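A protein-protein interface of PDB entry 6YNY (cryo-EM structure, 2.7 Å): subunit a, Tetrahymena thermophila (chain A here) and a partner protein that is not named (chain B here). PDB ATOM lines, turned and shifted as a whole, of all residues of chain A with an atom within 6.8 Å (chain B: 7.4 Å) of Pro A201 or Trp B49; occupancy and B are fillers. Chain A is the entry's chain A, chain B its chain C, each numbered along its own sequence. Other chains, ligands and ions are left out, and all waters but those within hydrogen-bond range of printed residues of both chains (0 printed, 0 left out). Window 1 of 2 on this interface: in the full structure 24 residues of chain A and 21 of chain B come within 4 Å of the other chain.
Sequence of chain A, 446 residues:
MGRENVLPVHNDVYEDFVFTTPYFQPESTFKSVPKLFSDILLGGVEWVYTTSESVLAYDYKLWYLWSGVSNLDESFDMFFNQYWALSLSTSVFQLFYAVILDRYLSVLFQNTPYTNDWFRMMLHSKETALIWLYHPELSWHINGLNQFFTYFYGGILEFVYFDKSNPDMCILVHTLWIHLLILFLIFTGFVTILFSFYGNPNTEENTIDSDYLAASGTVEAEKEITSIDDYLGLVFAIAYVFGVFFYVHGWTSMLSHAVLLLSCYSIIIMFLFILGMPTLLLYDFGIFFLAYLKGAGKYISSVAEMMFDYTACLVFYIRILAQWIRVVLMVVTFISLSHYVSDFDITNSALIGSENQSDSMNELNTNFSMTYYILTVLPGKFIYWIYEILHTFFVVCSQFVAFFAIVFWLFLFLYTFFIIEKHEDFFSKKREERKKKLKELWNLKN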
ATOM      1  N   PHE A 197     -14.917  22.524  14.385  1.00  0.00           N
ATOM      2  CA  PHE A 197     -14.449  22.398  13.014  1.00  0.00           C
ATOM      3  C   PHE A 197     -13.816  23.708  12.576  1.00  0.00           C
ATOM      4  O   PHE A 197     -14.112  24.220  11.493  1.00  0.00           O
ATOM      5  CB  PHE A 197     -15.604  22.021  12.094  1.00  0.00           C
ATOM      6  CG  PHE A 197     -16.577  21.067  12.708  1.00  0.00           C
ATOM      7  CD1 PHE A 197     -16.235  19.746  12.918  1.00  0.00           C
ATOM      8  CD2 PHE A 197     -17.838  21.491  13.073  1.00  0.00           C
ATOM      9  CE1 PHE A 197     -17.129  18.873  13.481  1.00  0.00           C
ATOM     10  CE2 PHE A 197     -18.734  20.619  13.636  1.00  0.00           C
ATOM     11  CZ  PHE A 197     -18.378  19.307  13.840  1.00  0.00           C
ATOM     12  N   TYR A 198     -12.951  24.255  13.423  1.00  0.00           N
ATOM     13  CA  TYR A 198     -12.348  25.570  13.219  1.00  0.00           C
ATOM     14  C   TYR A 198     -10.833  25.406  13.281  1.00  0.00           C
ATOM     15  O   TYR A 198     -10.204  25.630  14.315  1.00  0.00           O
ATOM     16  CB  TYR A 198     -12.866  26.532  14.259  1.00  0.00           C
ATOM     17  CG  TYR A 198     -14.304  26.270  14.625  1.00  0.00           C
ATOM     18  CD1 TYR A 198     -15.325  26.492  13.718  1.00  0.00           C
ATOM     19  CD2 TYR A 198     -14.639  25.786  15.877  1.00  0.00           C
ATOM     20  CE1 TYR A 198     -16.629  26.245  14.049  1.00  0.00           C
ATOM     21  CE2 TYR A 198     -15.942  25.538  16.215  1.00  0.00           C
ATOM     22  CZ  TYR A 198     -16.933  25.769  15.300  1.00  0.00           C
ATOM     23  OH  TYR A 198     -18.237  25.520  15.639  1.00  0.00           O
ATOM     24  N   GLY A 199     -10.250  25.028  12.153  1.00  0.00           N
ATOM     25  CA  GLY A 199      -8.825  24.804  12.060  1.00  0.00           C
ATOM     26  C   GLY A 199      -8.429  24.374  10.666  1.00  0.00           C
ATOM     27  O   GLY A 199      -8.901  24.948   9.680  1.00  0.00           O
ATOM     28  N   ASN A 200      -7.561  23.369  10.566  1.00  0.00           N
ATOM     29  CA  ASN A 200      -7.191  22.816   9.273  1.00  0.00           C
ATOM     30  C   ASN A 200      -8.122  21.651   8.964  1.00  0.00           C
ATOM     31  O   ASN A 200      -8.015  20.601   9.613  1.00  0.00           O
ATOM     32  CB  ASN A 200      -5.745  22.356   9.270  1.00  0.00           C
ATOM     33  CG  ASN A 200      -5.284  21.898   7.902  1.00  0.00           C
ATOM     34  OD1 ASN A 200      -6.079  21.442   7.085  1.00  0.00           O
ATOM     35  ND2 ASN A 200      -3.991  22.019   7.646  1.00  0.00           N
ATOM     36  N   PRO A 201      -9.040  21.782   8.004  1.00  0.00           N
ATOM     37  CA  PRO A 201      -9.966  20.683   7.708  1.00  0.00           C
ATOM     38  C   PRO A 201      -9.328  19.519   6.978  1.00  0.00           C
ATOM     39  O   PRO A 201     -10.016  18.527   6.714  1.00  0.00           O
ATOM     40  CB  PRO A 201     -11.029  21.360   6.838  1.00  0.00           C
ATOM     41  CG  PRO A 201     -10.314  22.457   6.177  1.00  0.00           C
ATOM     42  CD  PRO A 201      -9.288  22.949   7.144  1.00  0.00           C
ATOM     43  N   ASN A 202      -8.043  19.602   6.648  1.00  0.00           N
ATOM     44  CA  ASN A 202      -7.358  18.559   5.907  1.00  0.00           C
ATOM     45  C   ASN A 202      -6.405  17.739   6.762  1.00  0.00           C
ATOM     46  O   ASN A 202      -5.883  16.729   6.279  1.00  0.00           O
ATOM     47  CB  ASN A 202      -6.595  19.179   4.732  1.00  0.00           C
ATOM     48  CG  ASN A 202      -7.477  20.047   3.869  1.00  0.00           C
ATOM     49  OD1 ASN A 202      -8.578  19.651   3.492  1.00  0.00           O
ATOM     50  ND2 ASN A 202      -7.006  21.246   3.563  1.00  0.00           N
ATOM     51  N   THR A 203      -6.165  18.141   8.006  1.00  0.00           N
ATOM     52  CA  THR A 203      -5.333  17.391   8.933  1.00  0.00           C
ATOM     53  C   THR A 203      -6.096  16.861  10.132  1.00  0.00           C
ATOM     54  O   THR A 203      -5.728  15.813  10.665  1.00  0.00           O
ATOM     55  CB  THR A 203      -4.179  18.260   9.455  1.00  0.00           C
ATOM     56  OG1 THR A 203      -4.707  19.383  10.166  1.00  0.00           O
ATOM     57  CG2 THR A 203      -3.323  18.745   8.316  1.00  0.00           C
ATOM     58  N   GLU A 204      -7.142  17.553  10.569  1.00  0.00           N
ATOM     59  CA  GLU A 204      -7.911  17.140  11.734  1.00  0.00           C
ATOM     60  C   GLU A 204      -8.947  16.114  11.298  1.00  0.00           C
ATOM     61  O   GLU A 204      -9.937  16.456  10.643  1.00  0.00           O
ATOM     62  CB  GLU A 204      -8.559  18.354  12.389  1.00  0.00           C
ATOM     63  CG  GLU A 204      -7.560  19.416  12.797  1.00  0.00           C
ATOM     64  CD  GLU A 204      -8.214  20.652  13.376  1.00  0.00           C
ATOM     65  OE1 GLU A 204      -9.461  20.703  13.414  1.00  0.00           O
ATOM     66  OE2 GLU A 204      -7.481  21.573  13.788  1.00  0.00           O
ATOM     67  N   GLU A 205      -8.721  14.853  11.664  1.00  0.00           N
ATOM     68  CA  GLU A 205      -9.617  13.780  11.256  1.00  0.00           C
ATOM     69  C   GLU A 205     -11.013  13.940  11.831  1.00  0.00           C
ATOM     70  O   GLU A 205     -11.950  13.302  11.341  1.00  0.00           O
ATOM     71  CB  GLU A 205      -9.033  12.435  11.676  1.00  0.00           C
ATOM     72  CG  GLU A 205      -7.836  11.998  10.857  1.00  0.00           C
ATOM     73  CD  GLU A 205      -7.325  10.637  11.266  1.00  0.00           C
ATOM     74  OE1 GLU A 205      -6.098  10.484  11.431  1.00  0.00           O
ATOM     75  OE2 GLU A 205      -8.155   9.718  11.428  1.00  0.00           O
ATOM     76  N   THR A 207     -12.928  16.808  11.918  1.00  0.00           N
ATOM     77  CA  THR A 207     -13.724  17.551  10.951  1.00  0.00           C
ATOM     78  C   THR A 207     -13.749  16.878   9.588  1.00  0.00           C
ATOM     79  O   THR A 207     -14.684  17.107   8.816  1.00  0.00           O
ATOM     80  CB  THR A 207     -13.197  18.981  10.809  1.00  0.00           C
ATOM     81  OG1 THR A 207     -14.023  19.711   9.897  1.00  0.00           O
ATOM     82  CG2 THR A 207     -11.802  18.991  10.288  1.00  0.00           C
ATOM     83  N   ILE A 208     -12.747  16.057   9.277  1.00  0.00           N
ATOM     84  CA  ILE A 208     -12.766  15.290   8.037  1.00  0.00           C
ATOM     85  C   ILE A 208     -13.911  14.288   8.052  1.00  0.00           C
ATOM     86  O   ILE A 208     -14.702  14.207   7.107  1.00  0.00           O
ATOM     87  CB  ILE A 208     -11.411  14.594   7.828  1.00  0.00           C
ATOM     88  CG1 ILE A 208     -10.332  15.629   7.518  1.00  0.00           C
ATOM     89  CG2 ILE A 208     -11.509  13.560   6.731  1.00  0.00           C
ATOM     90  CD1 ILE A 208      -8.937  15.101   7.609  1.00  0.00           C
ATOM     91  N   ASP A 211     -17.327  16.160   8.038  1.00  0.00           N
ATOM     92  CA  ASP A 211     -17.603  16.922   6.827  1.00  0.00           C
ATOM     93  C   ASP A 211     -17.979  16.007   5.671  1.00  0.00           C
ATOM     94  O   ASP A 211     -19.000  16.216   5.007  1.00  0.00           O
ATOM     95  CB  ASP A 211     -16.389  17.772   6.462  1.00  0.00           C
ATOM     96  CG  ASP A 211     -16.643  18.667   5.277  1.00  0.00           C
ATOM     97  OD1 ASP A 211     -17.805  18.763   4.835  1.00  0.00           O
ATOM     98  OD2 ASP A 211     -15.675  19.275   4.779  1.00  0.00           O
ATOM     99  N   TYR A 212     -17.157  14.992   5.408  1.00  0.00           N
ATOM    100  CA  TYR A 212     -17.449  14.077   4.313  1.00  0.00           C
ATOM    101  C   TYR A 212     -18.687  13.236   4.596  1.00  0.00           C
ATOM    102  O   TYR A 212     -19.436  12.911   3.670  1.00  0.00           O
ATOM    103  CB  TYR A 212     -16.241  13.182   4.057  1.00  0.00           C
ATOM    104  CG  TYR A 212     -15.073  13.891   3.418  1.00  0.00           C
ATOM    105  CD1 TYR A 212     -14.791  13.735   2.073  1.00  0.00           C
ATOM    106  CD2 TYR A 212     -14.250  14.714   4.161  1.00  0.00           C
ATOM    107  CE1 TYR A 212     -13.724  14.381   1.491  1.00  0.00           C
ATOM    108  CE2 TYR A 212     -13.185  15.363   3.590  1.00  0.00           C
ATOM    109  CZ  TYR A 212     -12.925  15.194   2.255  1.00  0.00           C
ATOM    110  OH  TYR A 212     -11.859  15.845   1.685  1.00  0.00           O
ATOM    111  N   VAL B  44     -23.888  20.191  10.115  1.00  0.00           N
ATOM    112  CA  VAL B  44     -24.232  20.200   8.697  1.00  0.00           C
ATOM    113  C   VAL B  44     -24.047  21.593   8.116  1.00  0.00           C
ATOM    114  O   VAL B  44     -23.346  21.782   7.115  1.00  0.00           O
ATOM    115  CB  VAL B  44     -25.672  19.698   8.501  1.00  0.00           C
ATOM    116  CG1 VAL B  44     -26.114  19.891   7.070  1.00  0.00           C
ATOM    117  CG2 VAL B  44     -25.785  18.246   8.908  1.00  0.00           C
ATOM    118  N   VAL B  45     -24.673  22.592   8.737  1.00  0.00           N
ATOM    119  CA  VAL B  45     -24.688  23.931   8.167  1.00  0.00           C
ATOM    120  C   VAL B  45     -23.315  24.582   8.245  1.00  0.00           C
ATOM    121  O   VAL B  45     -22.948  25.374   7.368  1.00  0.00           O
ATOM    122  CB  VAL B  45     -25.763  24.771   8.871  1.00  0.00           C
ATOM    123  CG1 VAL B  45     -25.784  26.178   8.325  1.00  0.00           C
ATOM    124  CG2 VAL B  45     -27.110  24.107   8.704  1.00  0.00           C
ATOM    125  N   GLU B  46     -22.535  24.273   9.279  1.00  0.00           N
ATOM    126  CA  GLU B  46     -21.216  24.879   9.415  1.00  0.00           C
ATOM    127  C   GLU B  46     -20.209  24.274   8.448  1.00  0.00           C
ATOM    128  O   GLU B  46     -19.357  24.990   7.913  1.00  0.00           O
ATOM    129  CB  GLU B  46     -20.708  24.729  10.845  1.00  0.00           C
ATOM    130  CG  GLU B  46     -21.437  25.588  11.853  1.00  0.00           C
ATOM    131  CD  GLU B  46     -20.967  25.346  13.273  1.00  0.00           C
ATOM    132  OE1 GLU B  46     -19.822  24.885  13.450  1.00  0.00           O
ATOM    133  OE2 GLU B  46     -21.744  25.611  14.213  1.00  0.00           O
ATOM    134  N   LEU B  47     -20.295  22.971   8.198  1.00  0.00           N
ATOM    135  CA  LEU B  47     -19.263  22.261   7.459  1.00  0.00           C
ATOM    136  C   LEU B  47     -19.414  22.374   5.956  1.00  0.00           C
ATOM    137  O   LEU B  47     -18.893  21.525   5.225  1.00  0.00           O
ATOM    138  CB  LEU B  47     -19.238  20.791   7.877  1.00  0.00           C
ATOM    139  CG  LEU B  47     -18.540  20.542   9.211  1.00  0.00           C
ATOM    140  CD1 LEU B  47     -18.619  19.093   9.592  1.00  0.00           C
ATOM    141  CD2 LEU B  47     -17.101  20.988   9.135  1.00  0.00           C
ATOM    142  N   ILE B  48     -20.116  23.399   5.471  1.00  0.00           N
ATOM    143  CA  ILE B  48     -20.088  23.717   4.049  1.00  0.00           C
ATOM    144  C   ILE B  48     -18.910  24.605   3.683  1.00  0.00           C
ATOM    145  O   ILE B  48     -18.652  24.810   2.488  1.00  0.00           O
ATOM    146  CB  ILE B  48     -21.392  24.407   3.604  1.00  0.00           C
ATOM    147  CG1 ILE B  48     -21.573  25.739   4.325  1.00  0.00           C
ATOM    148  CG2 ILE B  48     -22.579  23.515   3.875  1.00  0.00           C
ATOM    149  CD1 ILE B  48     -22.845  26.431   3.987  1.00  0.00           C
ATOM    150  N   TRP B  49     -18.182  25.134   4.666  1.00  0.00           N
ATOM    151  CA  TRP B  49     -17.108  26.080   4.391  1.00  0.00           C
ATOM    152  C   TRP B  49     -15.856  25.412   3.830  1.00  0.00           C
ATOM    153  O   TRP B  49     -15.180  26.016   2.989  1.00  0.00           O
ATOM    154  CB  TRP B  49     -16.770  26.891   5.647  1.00  0.00           C
ATOM    155  CG  TRP B  49     -15.965  26.204   6.707  1.00  0.00           C
ATOM    156  CD1 TRP B  49     -16.434  25.649   7.860  1.00  0.00           C
ATOM    157  CD2 TRP B  49     -14.546  26.024   6.728  1.00  0.00           C
ATOM    158  NE1 TRP B  49     -15.402  25.128   8.588  1.00  0.00           N
ATOM    159  CE2 TRP B  49     -14.231  25.345   7.916  1.00  0.00           C
ATOM    160  CE3 TRP B  49     -13.513  26.366   5.854  1.00  0.00           C
ATOM    161  CZ2 TRP B  49     -12.932  25.001   8.251  1.00  0.00           C
ATOM    162  CZ3 TRP B  49     -12.230  26.023   6.189  1.00  0.00           C
ATOM    163  CH2 TRP B  49     -11.947  25.349   7.376  1.00  0.00           C
ATOM    164  N   PRO B  50     -15.499  24.193   4.242  1.00  0.00           N
ATOM    165  CA  PRO B  50     -14.299  23.585   3.651  1.00  0.00           C
ATOM    166  C   PRO B  50     -14.436  23.358   2.159  1.00  0.00           C
ATOM    167  O   PRO B  50     -13.493  23.606   1.402  1.00  0.00           O
ATOM    168  CB  PRO B  50     -14.149  22.273   4.431  1.00  0.00           C
ATOM    169  CG  PRO B  50     -15.005  22.419   5.618  1.00  0.00           C
ATOM    170  CD  PRO B  50     -16.128  23.273   5.201  1.00  0.00           C
ATOM    171  N   THR B  51     -15.605  22.897   1.715  1.00  0.00           N
ATOM    172  CA  THR B  51     -15.856  22.739   0.288  1.00  0.00           C
ATOM    173  C   THR B  51     -15.832  24.082  -0.427  1.00  0.00           C
ATOM    174  O   THR B  51     -15.224  24.222  -1.493  1.00  0.00           O
ATOM    175  CB  THR B  51     -17.202  22.049   0.081  1.00  0.00           C
ATOM    176  OG1 THR B  51     -17.146  20.713   0.587  1.00  0.00           O
ATOM    177  CG2 THR B  51     -17.572  22.026  -1.378  1.00  0.00           C
ATOM    178  N   HIS B  52     -16.495  25.084   0.147  1.00  0.00           N
ATOM    179  CA  HIS B  52     -16.530  26.401  -0.473  1.00  0.00           C
ATOM    180  C   HIS B  52     -15.147  27.033  -0.502  1.00  0.00           C
ATOM    181  O   HIS B  52     -14.765  27.661  -1.496  1.00  0.00           O
ATOM    182  CB  HIS B  52     -17.511  27.290   0.279  1.00  0.00           C
ATOM    183  CG  HIS B  52     -17.627  28.671  -0.277  1.00  0.00           C
ATOM    184  ND1 HIS B  52     -17.104  29.774   0.358  1.00  0.00           N
ATOM    185  CD2 HIS B  52     -18.211  29.128  -1.409  1.00  0.00           C
ATOM    186  CE1 HIS B  52     -17.360  30.853  -0.358  1.00  0.00           C
ATOM    187  NE2 HIS B  52     -18.031  30.488  -1.436  1.00  0.00           N
ATOM    188  N   PHE B  53     -14.385  26.881   0.579  1.00  0.00           N
ATOM    189  CA  PHE B  53     -13.047  27.451   0.626  1.00  0.00           C
ATOM    190  C   PHE B  53     -12.131  26.797  -0.396  1.00  0.00           C
ATOM    191  O   PHE B  53     -11.267  27.465  -0.972  1.00  0.00           O
ATOM    192  CB  PHE B  53     -12.478  27.302   2.034  1.00  0.00           C
ATOM    193  CG  PHE B  53     -11.115  27.887   2.204  1.00  0.00           C
ATOM    194  CD1 PHE B  53     -10.938  29.253   2.276  1.00  0.00           C
ATOM    195  CD2 PHE B  53     -10.009  27.070   2.310  1.00  0.00           C
ATOM    196  CE1 PHE B  53      -9.689  29.790   2.434  1.00  0.00           C
ATOM    197  CE2 PHE B  53      -8.756  27.606   2.471  1.00  0.00           C
ATOM    198  CZ  PHE B  53      -8.596  28.969   2.533  1.00  0.00           C
ATOM    199  N   PHE B  54     -12.310  25.501  -0.638  1.00  0.00           N
ATOM    200  CA  PHE B  54     -11.452  24.775  -1.565  1.00  0.00           C
ATOM    201  C   PHE B  54     -11.824  25.056  -3.015  1.00  0.00           C
ATOM    202  O   PHE B  54     -10.955  25.360  -3.838  1.00  0.00           O
ATOM    203  CB  PHE B  54     -11.536  23.279  -1.275  1.00  0.00           C
ATOM    204  CG  PHE B  54     -10.701  22.440  -2.187  1.00  0.00           C
ATOM    205  CD1 PHE B  54      -9.363  22.248  -1.930  1.00  0.00           C
ATOM    206  CD2 PHE B  54     -11.254  21.839  -3.298  1.00  0.00           C
ATOM    207  CE1 PHE B  54      -8.595  21.481  -2.761  1.00  0.00           C
ATOM    208  CE2 PHE B  54     -10.490  21.072  -4.129  1.00  0.00           C
ATOM    209  CZ  PHE B  54      -9.158  20.891  -3.862  1.00  0.00           C
ATOM    210  N   ASN B  55     -13.111  24.956  -3.347  1.00  0.00           N
ATOM    211  CA  ASN B  55     -13.527  25.089  -4.739  1.00  0.00           C
ATOM    212  C   ASN B  55     -13.217  26.475  -5.284  1.00  0.00           C
ATOM    213  O   ASN B  55     -12.779  26.614  -6.432  1.00  0.00           O
ATOM    214  CB  ASN B  55     -15.016  24.781  -4.870  1.00  0.00           C
ATOM    215  CG  ASN B  55     -15.333  23.326  -4.619  1.00  0.00           C
ATOM    216  OD1 ASN B  55     -14.455  22.468  -4.660  1.00  0.00           O
ATOM    217  ND2 ASN B  55     -16.597  23.038  -4.368  1.00  0.00           N
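NE1 of Trp B49 sits at hydrogen-bond distance from O of Phe A197, 3.3 Å away.
OH of Tyr A198 sits at hydrogen-bond distance from OE1 of Glu B46.
The side-chain carboxylate of Asp A211 sits close to the backbone carbonyl oxygen of Leu B47, at 3.0 Å.
Of the 13 printed residues of chain A, 6 touch a printed residue of chain B.
Hydrophobic or aromatic side chains of chain A that line the printed part of chain B: Phe A197, Tyr A198 and Pro A201.
Printed residues of chain B that touch a printed residue of chain A: Glu B46, Leu B47, Trp B49 and Pro B50.
Among the printed residues, 9 pairs touch across the chains.
Of chain B, only Trp B49 (3.5 Å) comes within 4 Å of Pro A201.
Trp B49 touches just these residues of chain A: Phe A197 (3.3 Å), Gly A199 (3.8 Å) and Pro A201 (3.5 Å).
Of the printed residues of chain B, Asp A211 touches Leu B47 (3.0 Å) and Pro B50 (3.3 Å).
Printed residues of chain A within 4 Å of Pro B50: Asp A211.
Of the printed residues of chain B, Phe A197 touches Glu B46 (3.9 Å), Leu B47 (3.5 Å) and Trp B49 (3.3 Å).
Val B45 touches none of the printed residues of chain A.
The nearest residue of chain B that does not touch Pro A201 is Pro B50 (4.04 Å).
Among the printed residues, merely in contact across the chains: Phe A197 with Glu B46 (3.9 Å), Phe A197 with Leu B47 (3.5 Å), Gly A199 with Trp B49 (3.8 Å), Pro A201 with Trp B49 (3.5 Å), Thr A207 with Leu B47 (3.4 Å) and Asp A211 with Pro B50 (3.3 Å).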
